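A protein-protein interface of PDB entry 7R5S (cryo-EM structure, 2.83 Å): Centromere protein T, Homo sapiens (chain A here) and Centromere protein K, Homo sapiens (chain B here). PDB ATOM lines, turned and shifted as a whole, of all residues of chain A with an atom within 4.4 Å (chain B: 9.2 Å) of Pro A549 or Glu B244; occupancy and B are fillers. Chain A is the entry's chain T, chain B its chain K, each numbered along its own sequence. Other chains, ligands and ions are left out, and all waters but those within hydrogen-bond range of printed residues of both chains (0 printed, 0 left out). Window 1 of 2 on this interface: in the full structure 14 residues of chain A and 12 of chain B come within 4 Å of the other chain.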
ATOM      1  N   GLU A 536     -24.872 -13.517  -4.753  1.00  0.00           N
ATOM      2  CA  GLU A 536     -25.436 -12.204  -5.043  1.00  0.00           C
ATOM      3  C   GLU A 536     -25.797 -12.057  -6.515  1.00  0.00           C
ATOM      4  O   GLU A 536     -26.762 -11.361  -6.849  1.00  0.00           O
ATOM      5  CB  GLU A 536     -24.455 -11.106  -4.632  1.00  0.00           C
ATOM      6  CG  GLU A 536     -24.199 -11.023  -3.138  1.00  0.00           C
ATOM      7  CD  GLU A 536     -23.094 -10.045  -2.794  1.00  0.00           C
ATOM      8  OE1 GLU A 536     -22.635  -9.320  -3.702  1.00  0.00           O
ATOM      9  OE2 GLU A 536     -22.681 -10.002  -1.615  1.00  0.00           O
ATOM     10  N   ARG A 544     -30.596 -15.043  -0.390  1.00  0.00           N
ATOM     11  CA  ARG A 544     -29.430 -14.332   0.120  1.00  0.00           C
ATOM     12  C   ARG A 544     -29.564 -14.039   1.608  1.00  0.00           C
ATOM     13  O   ARG A 544     -28.560 -14.021   2.330  1.00  0.00           O
ATOM     14  CB  ARG A 544     -29.222 -13.033  -0.661  1.00  0.00           C
ATOM     15  CG  ARG A 544     -27.929 -12.308  -0.327  1.00  0.00           C
ATOM     16  CD  ARG A 544     -27.909 -10.905  -0.912  1.00  0.00           C
ATOM     17  NE  ARG A 544     -28.192 -10.904  -2.344  1.00  0.00           N
ATOM     18  CZ  ARG A 544     -28.160  -9.820  -3.110  1.00  0.00           C
ATOM     19  NH1 ARG A 544     -27.851  -8.643  -2.583  1.00  0.00           N
ATOM     20  NH2 ARG A 544     -28.433  -9.910  -4.405  1.00  0.00           N
ATOM     21  N   LEU A 547     -28.440 -17.371   3.143  1.00  0.00           N
ATOM     22  CA  LEU A 547     -27.092 -17.863   2.867  1.00  0.00           C
ATOM     23  C   LEU A 547     -26.012 -16.919   3.390  1.00  0.00           C
ATOM     24  O   LEU A 547     -25.170 -17.318   4.201  1.00  0.00           O
ATOM     25  CB  LEU A 547     -26.920 -18.098   1.362  1.00  0.00           C
ATOM     26  CG  LEU A 547     -27.767 -19.223   0.766  1.00  0.00           C
ATOM     27  CD1 LEU A 547     -27.456 -19.405  -0.708  1.00  0.00           C
ATOM     28  CD2 LEU A 547     -27.544 -20.519   1.527  1.00  0.00           C
ATOM     29  N   ILE A 548     -26.022 -15.673   2.938  1.00  0.00           N
ATOM     30  CA  ILE A 548     -24.953 -14.734   3.285  1.00  0.00           C
ATOM     31  C   ILE A 548     -25.270 -14.099   4.637  1.00  0.00           C
ATOM     32  O   ILE A 548     -26.399 -13.624   4.838  1.00  0.00           O
ATOM     33  CB  ILE A 548     -24.798 -13.672   2.202  1.00  0.00           C
ATOM     34  CG1 ILE A 548     -24.605 -14.332   0.836  1.00  0.00           C
ATOM     35  CG2 ILE A 548     -23.624 -12.760   2.515  1.00  0.00           C
ATOM     36  CD1 ILE A 548     -24.379 -13.349  -0.288  1.00  0.00           C
ATOM     37  N   PRO A 549     -24.323 -14.069   5.573  1.00  0.00           N
ATOM     38  CA  PRO A 549     -24.595 -13.446   6.874  1.00  0.00           C
ATOM     39  C   PRO A 549     -24.653 -11.931   6.767  1.00  0.00           C
ATOM     40  O   PRO A 549     -23.927 -11.315   5.983  1.00  0.00           O
ATOM     41  CB  PRO A 549     -23.415 -13.903   7.739  1.00  0.00           C
ATOM     42  CG  PRO A 549     -22.317 -14.152   6.762  1.00  0.00           C
ATOM     43  CD  PRO A 549     -22.980 -14.673   5.517  1.00  0.00           C
ATOM     44  N   CYS A 550     -25.530 -11.332   7.571  1.00  0.00           N
ATOM     45  CA  CYS A 550     -25.705  -9.887   7.591  1.00  0.00           C
ATOM     46  C   CYS A 550     -25.957  -9.431   9.019  1.00  0.00           C
ATOM     47  O   CYS A 550     -26.573 -10.153   9.808  1.00  0.00           O
ATOM     48  CB  CYS A 550     -26.863  -9.451   6.686  1.00  0.00           C
ATOM     49  SG  CYS A 550     -27.019  -7.663   6.484  1.00  0.00           S
ATOM     50  N   VAL A 557     -26.115 -10.520  14.107  1.00  0.00           N
ATOM     51  CA  VAL A 557     -25.670 -11.134  12.861  1.00  0.00           C
ATOM     52  C   VAL A 557     -26.485 -12.397  12.618  1.00  0.00           C
ATOM     53  O   VAL A 557     -26.662 -13.217  13.528  1.00  0.00           O
ATOM     54  CB  VAL A 557     -24.161 -11.438  12.893  1.00  0.00           C
ATOM     55  CG1 VAL A 557     -23.777 -12.113  14.204  1.00  0.00           C
ATOM     56  CG2 VAL A 557     -23.758 -12.296  11.704  1.00  0.00           C
ATOM     57  N   PHE A 558     -26.987 -12.548  11.390  1.00  0.00           N
ATOM     58  CA  PHE A 558     -27.761 -13.714  10.998  1.00  0.00           C
ATOM     59  C   PHE A 558     -27.458 -14.035   9.537  1.00  0.00           C
ATOM     60  O   PHE A 558     -27.533 -13.134   8.680  1.00  0.00           O
ATOM     61  CB  PHE A 558     -29.263 -13.491  11.195  1.00  0.00           C
ATOM     62  CG  PHE A 558     -30.112 -14.647  10.750  1.00  0.00           C
ATOM     63  CD1 PHE A 558     -30.241 -15.775  11.543  1.00  0.00           C
ATOM     64  CD2 PHE A 558     -30.783 -14.606   9.539  1.00  0.00           C
ATOM     65  CE1 PHE A 558     -31.021 -16.841  11.137  1.00  0.00           C
ATOM     66  CE2 PHE A 558     -31.565 -15.668   9.126  1.00  0.00           C
ATOM     67  CZ  PHE A 558     -31.684 -16.787   9.927  1.00  0.00           C
ATOM     68  N   PRO A 559     -27.101 -15.288   9.214  1.00  0.00           N
ATOM     69  CA  PRO A 559     -26.853 -16.368  10.178  1.00  0.00           C
ATOM     70  C   PRO A 559     -25.535 -16.190  10.928  1.00  0.00           C
ATOM     71  O   PRO A 559     -24.704 -15.381  10.518  1.00  0.00           O
ATOM     72  CB  PRO A 559     -26.811 -17.626   9.300  1.00  0.00           C
ATOM     73  CG  PRO A 559     -27.460 -17.231   8.013  1.00  0.00           C
ATOM     74  CD  PRO A 559     -27.118 -15.791   7.832  1.00  0.00           C
ATOM     75  N   GLN A 561     -22.099 -16.361  11.656  1.00  0.00           N
ATOM     76  CA  GLN A 561     -20.872 -16.700  10.945  1.00  0.00           C
ATOM     77  C   GLN A 561     -19.691 -15.900  11.484  1.00  0.00           C
ATOM     78  O   GLN A 561     -19.714 -14.669  11.488  1.00  0.00           O
ATOM     79  CB  GLN A 561     -21.033 -16.454   9.443  1.00  0.00           C
ATOM     80  CG  GLN A 561     -21.178 -17.721   8.616  1.00  0.00           C
ATOM     81  CD  GLN A 561     -22.529 -18.384   8.793  1.00  0.00           C
ATOM     82  OE1 GLN A 561     -23.525 -17.721   9.083  1.00  0.00           O
ATOM     83  NE2 GLN A 561     -22.571 -19.699   8.616  1.00  0.00           N
ATOM     84  N   LEU B 212     -19.417   1.754  11.076  1.00  0.00           N
ATOM     85  CA  LEU B 212     -20.061   1.938   9.780  1.00  0.00           C
ATOM     86  C   LEU B 212     -20.097   3.407   9.376  1.00  0.00           C
ATOM     87  O   LEU B 212     -20.081   3.722   8.179  1.00  0.00           O
ATOM     88  CB  LEU B 212     -21.475   1.357   9.814  1.00  0.00           C
ATOM     89  CG  LEU B 212     -22.292   1.395   8.523  1.00  0.00           C
ATOM     90  CD1 LEU B 212     -21.601   0.603   7.425  1.00  0.00           C
ATOM     91  CD2 LEU B 212     -23.697   0.867   8.765  1.00  0.00           C
ATOM     92  N   MET B 215     -16.975   4.258   7.467  1.00  0.00           N
ATOM     93  CA  MET B 215     -17.024   3.709   6.115  1.00  0.00           C
ATOM     94  C   MET B 215     -17.925   4.546   5.215  1.00  0.00           C
ATOM     95  O   MET B 215     -17.578   4.823   4.059  1.00  0.00           O
ATOM     96  CB  MET B 215     -17.506   2.259   6.158  1.00  0.00           C
ATOM     97  CG  MET B 215     -17.296   1.492   4.864  1.00  0.00           C
ATOM     98  SD  MET B 215     -18.161  -0.091   4.853  1.00  0.00           S
ATOM     99  CE  MET B 215     -17.765  -0.710   6.485  1.00  0.00           C
ATOM    100  N   ILE B 234     -11.677  -2.828  -0.775  1.00  0.00           N
ATOM    101  CA  ILE B 234     -12.136  -3.360   0.504  1.00  0.00           C
ATOM    102  C   ILE B 234     -10.934  -3.745   1.353  1.00  0.00           C
ATOM    103  O   ILE B 234     -10.023  -4.446   0.891  1.00  0.00           O
ATOM    104  CB  ILE B 234     -13.074  -4.555   0.284  1.00  0.00           C
ATOM    105  CG1 ILE B 234     -14.257  -4.151  -0.597  1.00  0.00           C
ATOM    106  CG2 ILE B 234     -13.565  -5.102   1.617  1.00  0.00           C
ATOM    107  CD1 ILE B 234     -15.225  -5.278  -0.884  1.00  0.00           C
ATOM    108  N   PHE B 238     -13.183  -3.296   6.966  1.00  0.00           N
ATOM    109  CA  PHE B 238     -14.541  -3.486   6.459  1.00  0.00           C
ATOM    110  C   PHE B 238     -14.882  -4.966   6.580  1.00  0.00           C
ATOM    111  O   PHE B 238     -14.597  -5.767   5.689  1.00  0.00           O
ATOM    112  CB  PHE B 238     -14.656  -3.010   5.016  1.00  0.00           C
ATOM    113  CG  PHE B 238     -14.167  -1.605   4.790  1.00  0.00           C
ATOM    114  CD1 PHE B 238     -14.285  -0.640   5.777  1.00  0.00           C
ATOM    115  CD2 PHE B 238     -13.590  -1.251   3.582  1.00  0.00           C
ATOM    116  CE1 PHE B 238     -13.836   0.649   5.561  1.00  0.00           C
ATOM    117  CE2 PHE B 238     -13.139   0.035   3.362  1.00  0.00           C
ATOM    118  CZ  PHE B 238     -13.262   0.986   4.353  1.00  0.00           C
ATOM    119  N   TRP B 239     -15.502  -5.339   7.699  1.00  0.00           N
ATOM    120  CA  TRP B 239     -15.812  -6.748   7.870  1.00  0.00           C
ATOM    121  C   TRP B 239     -17.057  -7.125   7.063  1.00  0.00           C
ATOM    122  O   TRP B 239     -17.888  -6.267   6.754  1.00  0.00           O
ATOM    123  CB  TRP B 239     -15.998  -7.085   9.352  1.00  0.00           C
ATOM    124  CG  TRP B 239     -17.241  -6.561  10.003  1.00  0.00           C
ATOM    125  CD1 TRP B 239     -17.953  -5.452   9.654  1.00  0.00           C
ATOM    126  CD2 TRP B 239     -17.910  -7.127  11.138  1.00  0.00           C
ATOM    127  NE1 TRP B 239     -19.028  -5.297  10.495  1.00  0.00           N
ATOM    128  CE2 TRP B 239     -19.024  -6.312  11.415  1.00  0.00           C
ATOM    129  CE3 TRP B 239     -17.677  -8.246  11.943  1.00  0.00           C
ATOM    130  CZ2 TRP B 239     -19.903  -6.581  12.463  1.00  0.00           C
ATOM    131  CZ3 TRP B 239     -18.550  -8.511  12.982  1.00  0.00           C
ATOM    132  CH2 TRP B 239     -19.650  -7.681  13.233  1.00  0.00           C
ATOM    133  N   PRO B 240     -17.186  -8.398   6.690  1.00  0.00           N
ATOM    134  CA  PRO B 240     -18.245  -8.816   5.749  1.00  0.00           C
ATOM    135  C   PRO B 240     -19.648  -8.410   6.181  1.00  0.00           C
ATOM    136  O   PRO B 240     -20.480  -8.123   5.308  1.00  0.00           O
ATOM    137  CB  PRO B 240     -18.096 -10.349   5.700  1.00  0.00           C
ATOM    138  CG  PRO B 240     -16.970 -10.701   6.651  1.00  0.00           C
ATOM    139  CD  PRO B 240     -16.179  -9.456   6.869  1.00  0.00           C
ATOM    140  N   PRO B 241     -19.984  -8.400   7.482  1.00  0.00           N
ATOM    141  CA  PRO B 241     -21.353  -7.976   7.847  1.00  0.00           C
ATOM    142  C   PRO B 241     -21.754  -6.604   7.323  1.00  0.00           C
ATOM    143  O   PRO B 241     -22.800  -6.479   6.669  1.00  0.00           O
ATOM    144  CB  PRO B 241     -21.320  -8.020   9.378  1.00  0.00           C
ATOM    145  CG  PRO B 241     -20.408  -9.125   9.673  1.00  0.00           C
ATOM    146  CD  PRO B 241     -19.317  -9.031   8.640  1.00  0.00           C
ATOM    147  N   TYR B 242     -20.959  -5.565   7.591  1.00  0.00           N
ATOM    148  CA  TYR B 242     -21.349  -4.217   7.184  1.00  0.00           C
ATOM    149  C   TYR B 242     -21.334  -4.065   5.668  1.00  0.00           C
ATOM    150  O   TYR B 242     -22.203  -3.395   5.095  1.00  0.00           O
ATOM    151  CB  TYR B 242     -20.431  -3.181   7.834  1.00  0.00           C
ATOM    152  CG  TYR B 242     -20.672  -2.985   9.313  1.00  0.00           C
ATOM    153  CD1 TYR B 242     -21.792  -3.523   9.933  1.00  0.00           C
ATOM    154  CD2 TYR B 242     -19.780  -2.258  10.090  1.00  0.00           C
ATOM    155  CE1 TYR B 242     -22.014  -3.346  11.285  1.00  0.00           C
ATOM    156  CE2 TYR B 242     -19.994  -2.076  11.443  1.00  0.00           C
ATOM    157  CZ  TYR B 242     -21.113  -2.623  12.035  1.00  0.00           C
ATOM    158  OH  TYR B 242     -21.330  -2.443  13.381  1.00  0.00           O
ATOM    159  N   VAL B 243     -20.351  -4.674   5.001  1.00  0.00           N
ATOM    160  CA  VAL B 243     -20.289  -4.606   3.544  1.00  0.00           C
ATOM    161  C   VAL B 243     -21.512  -5.273   2.931  1.00  0.00           C
ATOM    162  O   VAL B 243     -22.113  -4.752   1.983  1.00  0.00           O
ATOM    163  CB  VAL B 243     -18.982  -5.240   3.034  1.00  0.00           C
ATOM    164  CG1 VAL B 243     -18.894  -5.133   1.519  1.00  0.00           C
ATOM    165  CG2 VAL B 243     -17.781  -4.577   3.690  1.00  0.00           C
ATOM    166  N   GLU B 244     -21.906  -6.431   3.466  1.00  0.00           N
ATOM    167  CA  GLU B 244     -23.092  -7.114   2.965  1.00  0.00           C
ATOM    168  C   GLU B 244     -24.349  -6.297   3.226  1.00  0.00           C
ATOM    169  O   GLU B 244     -25.246  -6.244   2.377  1.00  0.00           O
ATOM    170  CB  GLU B 244     -23.209  -8.500   3.598  1.00  0.00           C
ATOM    171  CG  GLU B 244     -24.510  -9.221   3.284  1.00  0.00           C
ATOM    172  CD  GLU B 244     -24.688  -9.491   1.801  1.00  0.00           C
ATOM    173  OE1 GLU B 244     -23.670  -9.672   1.100  1.00  0.00           O
ATOM    174  OE2 GLU B 244     -25.847  -9.524   1.338  1.00  0.00           O
ATOM    175  N   LEU B 245     -24.434  -5.651   4.391  1.00  0.00           N
ATOM    176  CA  LEU B 245     -25.575  -4.786   4.678  1.00  0.00           C
ATOM    177  C   LEU B 245     -25.675  -3.658   3.658  1.00  0.00           C
ATOM    178  O   LEU B 245     -26.749  -3.399   3.097  1.00  0.00           O
ATOM    179  CB  LEU B 245     -25.460  -4.225   6.095  1.00  0.00           C
ATOM    180  CG  LEU B 245     -26.589  -3.305   6.565  1.00  0.00           C
ATOM    181  CD1 LEU B 245     -27.869  -4.094   6.777  1.00  0.00           C
ATOM    182  CD2 LEU B 245     -26.190  -2.572   7.835  1.00  0.00           C
ATOM    183  N   LEU B 246     -24.555  -2.977   3.402  1.00  0.00           N
ATOM    184  CA  LEU B 246     -24.564  -1.860   2.462  1.00  0.00           C
ATOM    185  C   LEU B 246     -24.877  -2.325   1.045  1.00  0.00           C
ATOM    186  O   LEU B 246     -25.565  -1.626   0.293  1.00  0.00           O
ATOM    187  CB  LEU B 246     -23.223  -1.128   2.502  1.00  0.00           C
ATOM    188  CG  LEU B 246     -22.884  -0.401   3.804  1.00  0.00           C
ATOM    189  CD1 LEU B 246     -21.583   0.371   3.660  1.00  0.00           C
ATOM    190  CD2 LEU B 246     -24.016   0.526   4.216  1.00  0.00           C
ATOM    191  N   LEU B 247     -24.381  -3.504   0.660  1.00  0.00           N
ATOM    192  CA  LEU B 247     -24.650  -4.007  -0.683  1.00  0.00           C
ATOM    193  C   LEU B 247     -26.089  -4.480  -0.832  1.00  0.00           C
ATOM    194  O   LEU B 247     -26.659  -4.394  -1.926  1.00  0.00           O
ATOM    195  CB  LEU B 247     -23.682  -5.139  -1.024  1.00  0.00           C
ATOM    196  CG  LEU B 247     -22.222  -4.743  -1.250  1.00  0.00           C
ATOM    197  CD1 LEU B 247     -21.354  -5.976  -1.417  1.00  0.00           C
ATOM    198  CD2 LEU B 247     -22.096  -3.830  -2.457  1.00  0.00           C
ATOM    199  N   ARG B 248     -26.693  -4.980   0.248  1.00  0.00           N
ATOM    200  CA  ARG B 248     -28.068  -5.458   0.182  1.00  0.00           C
ATOM    201  C   ARG B 248     -29.062  -4.305   0.198  1.00  0.00           C
ATOM    202  O   ARG B 248     -30.097  -4.367  -0.473  1.00  0.00           O
ATOM    203  CB  ARG B 248     -28.342  -6.417   1.342  1.00  0.00           C
ATOM    204  CG  ARG B 248     -29.710  -7.073   1.302  1.00  0.00           C
ATOM    205  CD  ARG B 248     -29.924  -7.963   2.515  1.00  0.00           C
ATOM    206  NE  ARG B 248     -28.885  -8.982   2.632  1.00  0.00           N
ATOM    207  CZ  ARG B 248     -28.817  -9.869   3.618  1.00  0.00           C
ATOM    208  NH1 ARG B 248     -29.729  -9.867   4.580  1.00  0.00           N
ATOM    209  NH2 ARG B 248     -27.837 -10.761   3.644  1.00  0.00           N
ATOM    210  N   ASN B 249     -28.767  -3.247   0.952  1.00  0.00           N
ATOM    211  CA  ASN B 249     -29.665  -2.102   1.024  1.00  0.00           C
ATOM    212  C   ASN B 249     -29.496  -1.136  -0.144  1.00  0.00           C
ATOM    213  O   ASN B 249     -30.077  -0.046  -0.112  1.00  0.00           O
ATOM    214  CB  ASN B 249     -29.467  -1.361   2.347  1.00  0.00           C
ATOM    215  CG  ASN B 249     -29.957  -2.161   3.534  1.00  0.00           C
ATOM    216  OD1 ASN B 249     -29.315  -2.195   4.583  1.00  0.00           O
ATOM    217  ND2 ASN B 249     -31.099  -2.819   3.372  1.00  0.00           N
ATOM    218  N   GLY B 250     -28.724  -1.503  -1.163  1.00  0.00           N
ATOM    219  CA  GLY B 250     -28.557  -0.662  -2.331  1.00  0.00           C
ATOM    220  C   GLY B 250     -27.718   0.577  -2.124  1.00  0.00           C
ATOM    221  O   GLY B 250     -27.674   1.430  -3.018  1.00  0.00           O
ATOM    222  N   ILE B 251     -27.048   0.707  -0.978  1.00  0.00           N
ATOM    223  CA  ILE B 251     -26.242   1.894  -0.722  1.00  0.00           C
ATOM    224  C   ILE B 251     -24.921   1.826  -1.479  1.00  0.00           C
ATOM    225  O   ILE B 251     -24.465   2.826  -2.044  1.00  0.00           O
ATOM    226  CB  ILE B 251     -26.022   2.066   0.791  1.00  0.00           C
ATOM    227  CG1 ILE B 251     -27.366   2.114   1.519  1.00  0.00           C
ATOM    228  CG2 ILE B 251     -25.221   3.325   1.076  1.00  0.00           C
ATOM    229  CD1 ILE B 251     -27.245   2.322   3.012  1.00  0.00           C
ATOM    230  N   ALA B 252     -24.291   0.655  -1.511  1.00  0.00           N
ATOM    231  CA  ALA B 252     -23.016   0.468  -2.183  1.00  0.00           C
ATOM    232  C   ALA B 252     -23.168  -0.513  -3.338  1.00  0.00           C
ATOM    233  O   ALA B 252     -24.123  -1.293  -3.399  1.00  0.00           O
ATOM    234  CB  ALA B 252     -21.940  -0.032  -1.210  1.00  0.00           C
ATOM    235  N   ARG B 254     -20.684  -3.123  -5.989  1.00  0.00           N
ATOM    236  CA  ARG B 254     -19.388  -3.708  -6.294  1.00  0.00           C
ATOM    237  C   ARG B 254     -18.919  -3.283  -7.680  1.00  0.00           C
ATOM    238  O   ARG B 254     -19.720  -2.945  -8.556  1.00  0.00           O
ATOM    239  CB  ARG B 254     -19.453  -5.234  -6.221  1.00  0.00           C
ATOM    240  CG  ARG B 254     -19.600  -5.800  -4.820  1.00  0.00           C
ATOM    241  CD  ARG B 254     -19.455  -7.315  -4.833  1.00  0.00           C
ATOM    242  NE  ARG B 254     -19.571  -7.895  -3.498  1.00  0.00           N
ATOM    243  CZ  ARG B 254     -18.559  -8.013  -2.645  1.00  0.00           C
ATOM    244  NH1 ARG B 254     -17.349  -7.587  -2.982  1.00  0.00           N
ATOM    245  NH2 ARG B 254     -18.757  -8.554  -1.451  1.00  0.00           N
ATOM    246  N   ILE B 262     -15.493  -1.290  -4.200  1.00  0.00           N
ATOM    247  CA  ILE B 262     -16.887  -0.891  -4.071  1.00  0.00           C
ATOM    248  C   ILE B 262     -16.986   0.623  -4.202  1.00  0.00           C
ATOM    249  O   ILE B 262     -16.031   1.359  -3.949  1.00  0.00           O
ATOM    250  CB  ILE B 262     -17.511  -1.357  -2.738  1.00  0.00           C
ATOM    251  CG1 ILE B 262     -16.693  -0.838  -1.554  1.00  0.00           C
ATOM    252  CG2 ILE B 262     -17.619  -2.874  -2.700  1.00  0.00           C
ATOM    253  CD1 ILE B 262     -17.239  -1.254  -0.206  1.00  0.00           C
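Of the printed residues of chain B, Arg A544 touches Glu B244 and Arg B248.
Of chain B, only Glu B244 (3.4 Å) and Arg B248 (3.4 Å) come within 4 Å of Ile A548.
Printed residues of chain B within 4 Å of Pro A549: Glu B244 (3.5 Å).
Cys A550 touches just these residues of chain B: Leu B245 (3.7 Å) and Arg B248 (3.5 Å).
Ile B234 touches none of the printed residues of chain A.
Glu B244 touches four residues of chain A.
Printed residues of chain A within 4 Å of Arg B248: Arg A544 (3.6 Å), Ile A548 (3.4 Å) and Cys A550 (3.5 Å).
The nearest residue of chain A that does not touch Glu B244 is Cys A550 (4.1 Å).
The nearest printed residue of chain A that does not touch Arg B248 is Pro A549 (4.6 Å).
Of the 10 printed residues of chain A, 5 touch a printed residue of chain B.
Printed residues of chain B that touch a printed residue of chain A: Glu B244, Leu B245, Arg B248 and Arg B254.
Hydrophobic or aromatic side chains of chain B within 4 Å of the printed part of chain A: Leu B245.
Among the printed residues, 9 pairs touch across the chains.
The backbone carbonyl oxygen (O) of Ile A548 lies within hydrogen-bond range of the guanidinium group (NH2) of Arg B248, 3.4 Å away.
OE1 of Glu A536 is in salt-bridge range of NE of Arg B254, at 3.4 Å.
OE2 of Glu A536 sits close to OE1 of Glu B244.
OD1 of Asn B249 lies close to O of Leu B245 (3.2 Å).
N of Phe A558 lies within hydrogen-bond range of O of Cys A550 (2.9 Å).
The guanidinium group of Arg A544 is in hydrogen-bond range of the backbone carbonyl oxygen of Glu A536 (3.3 Å).
The guanidinium group (NH2) of Arg B248 lies within salt-bridge range of the side-chain carboxylate (OE2) of Glu B244, 3.3 Å away.
Among the printed residues, pairs that only touch across the chains: Arg A544 with Glu B244, Arg A544 with Arg B248, Ile A548 with Glu B244, Pro A549 with Glu B244, Cys A550 with Leu B245 and Cys A550 with Arg B248.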
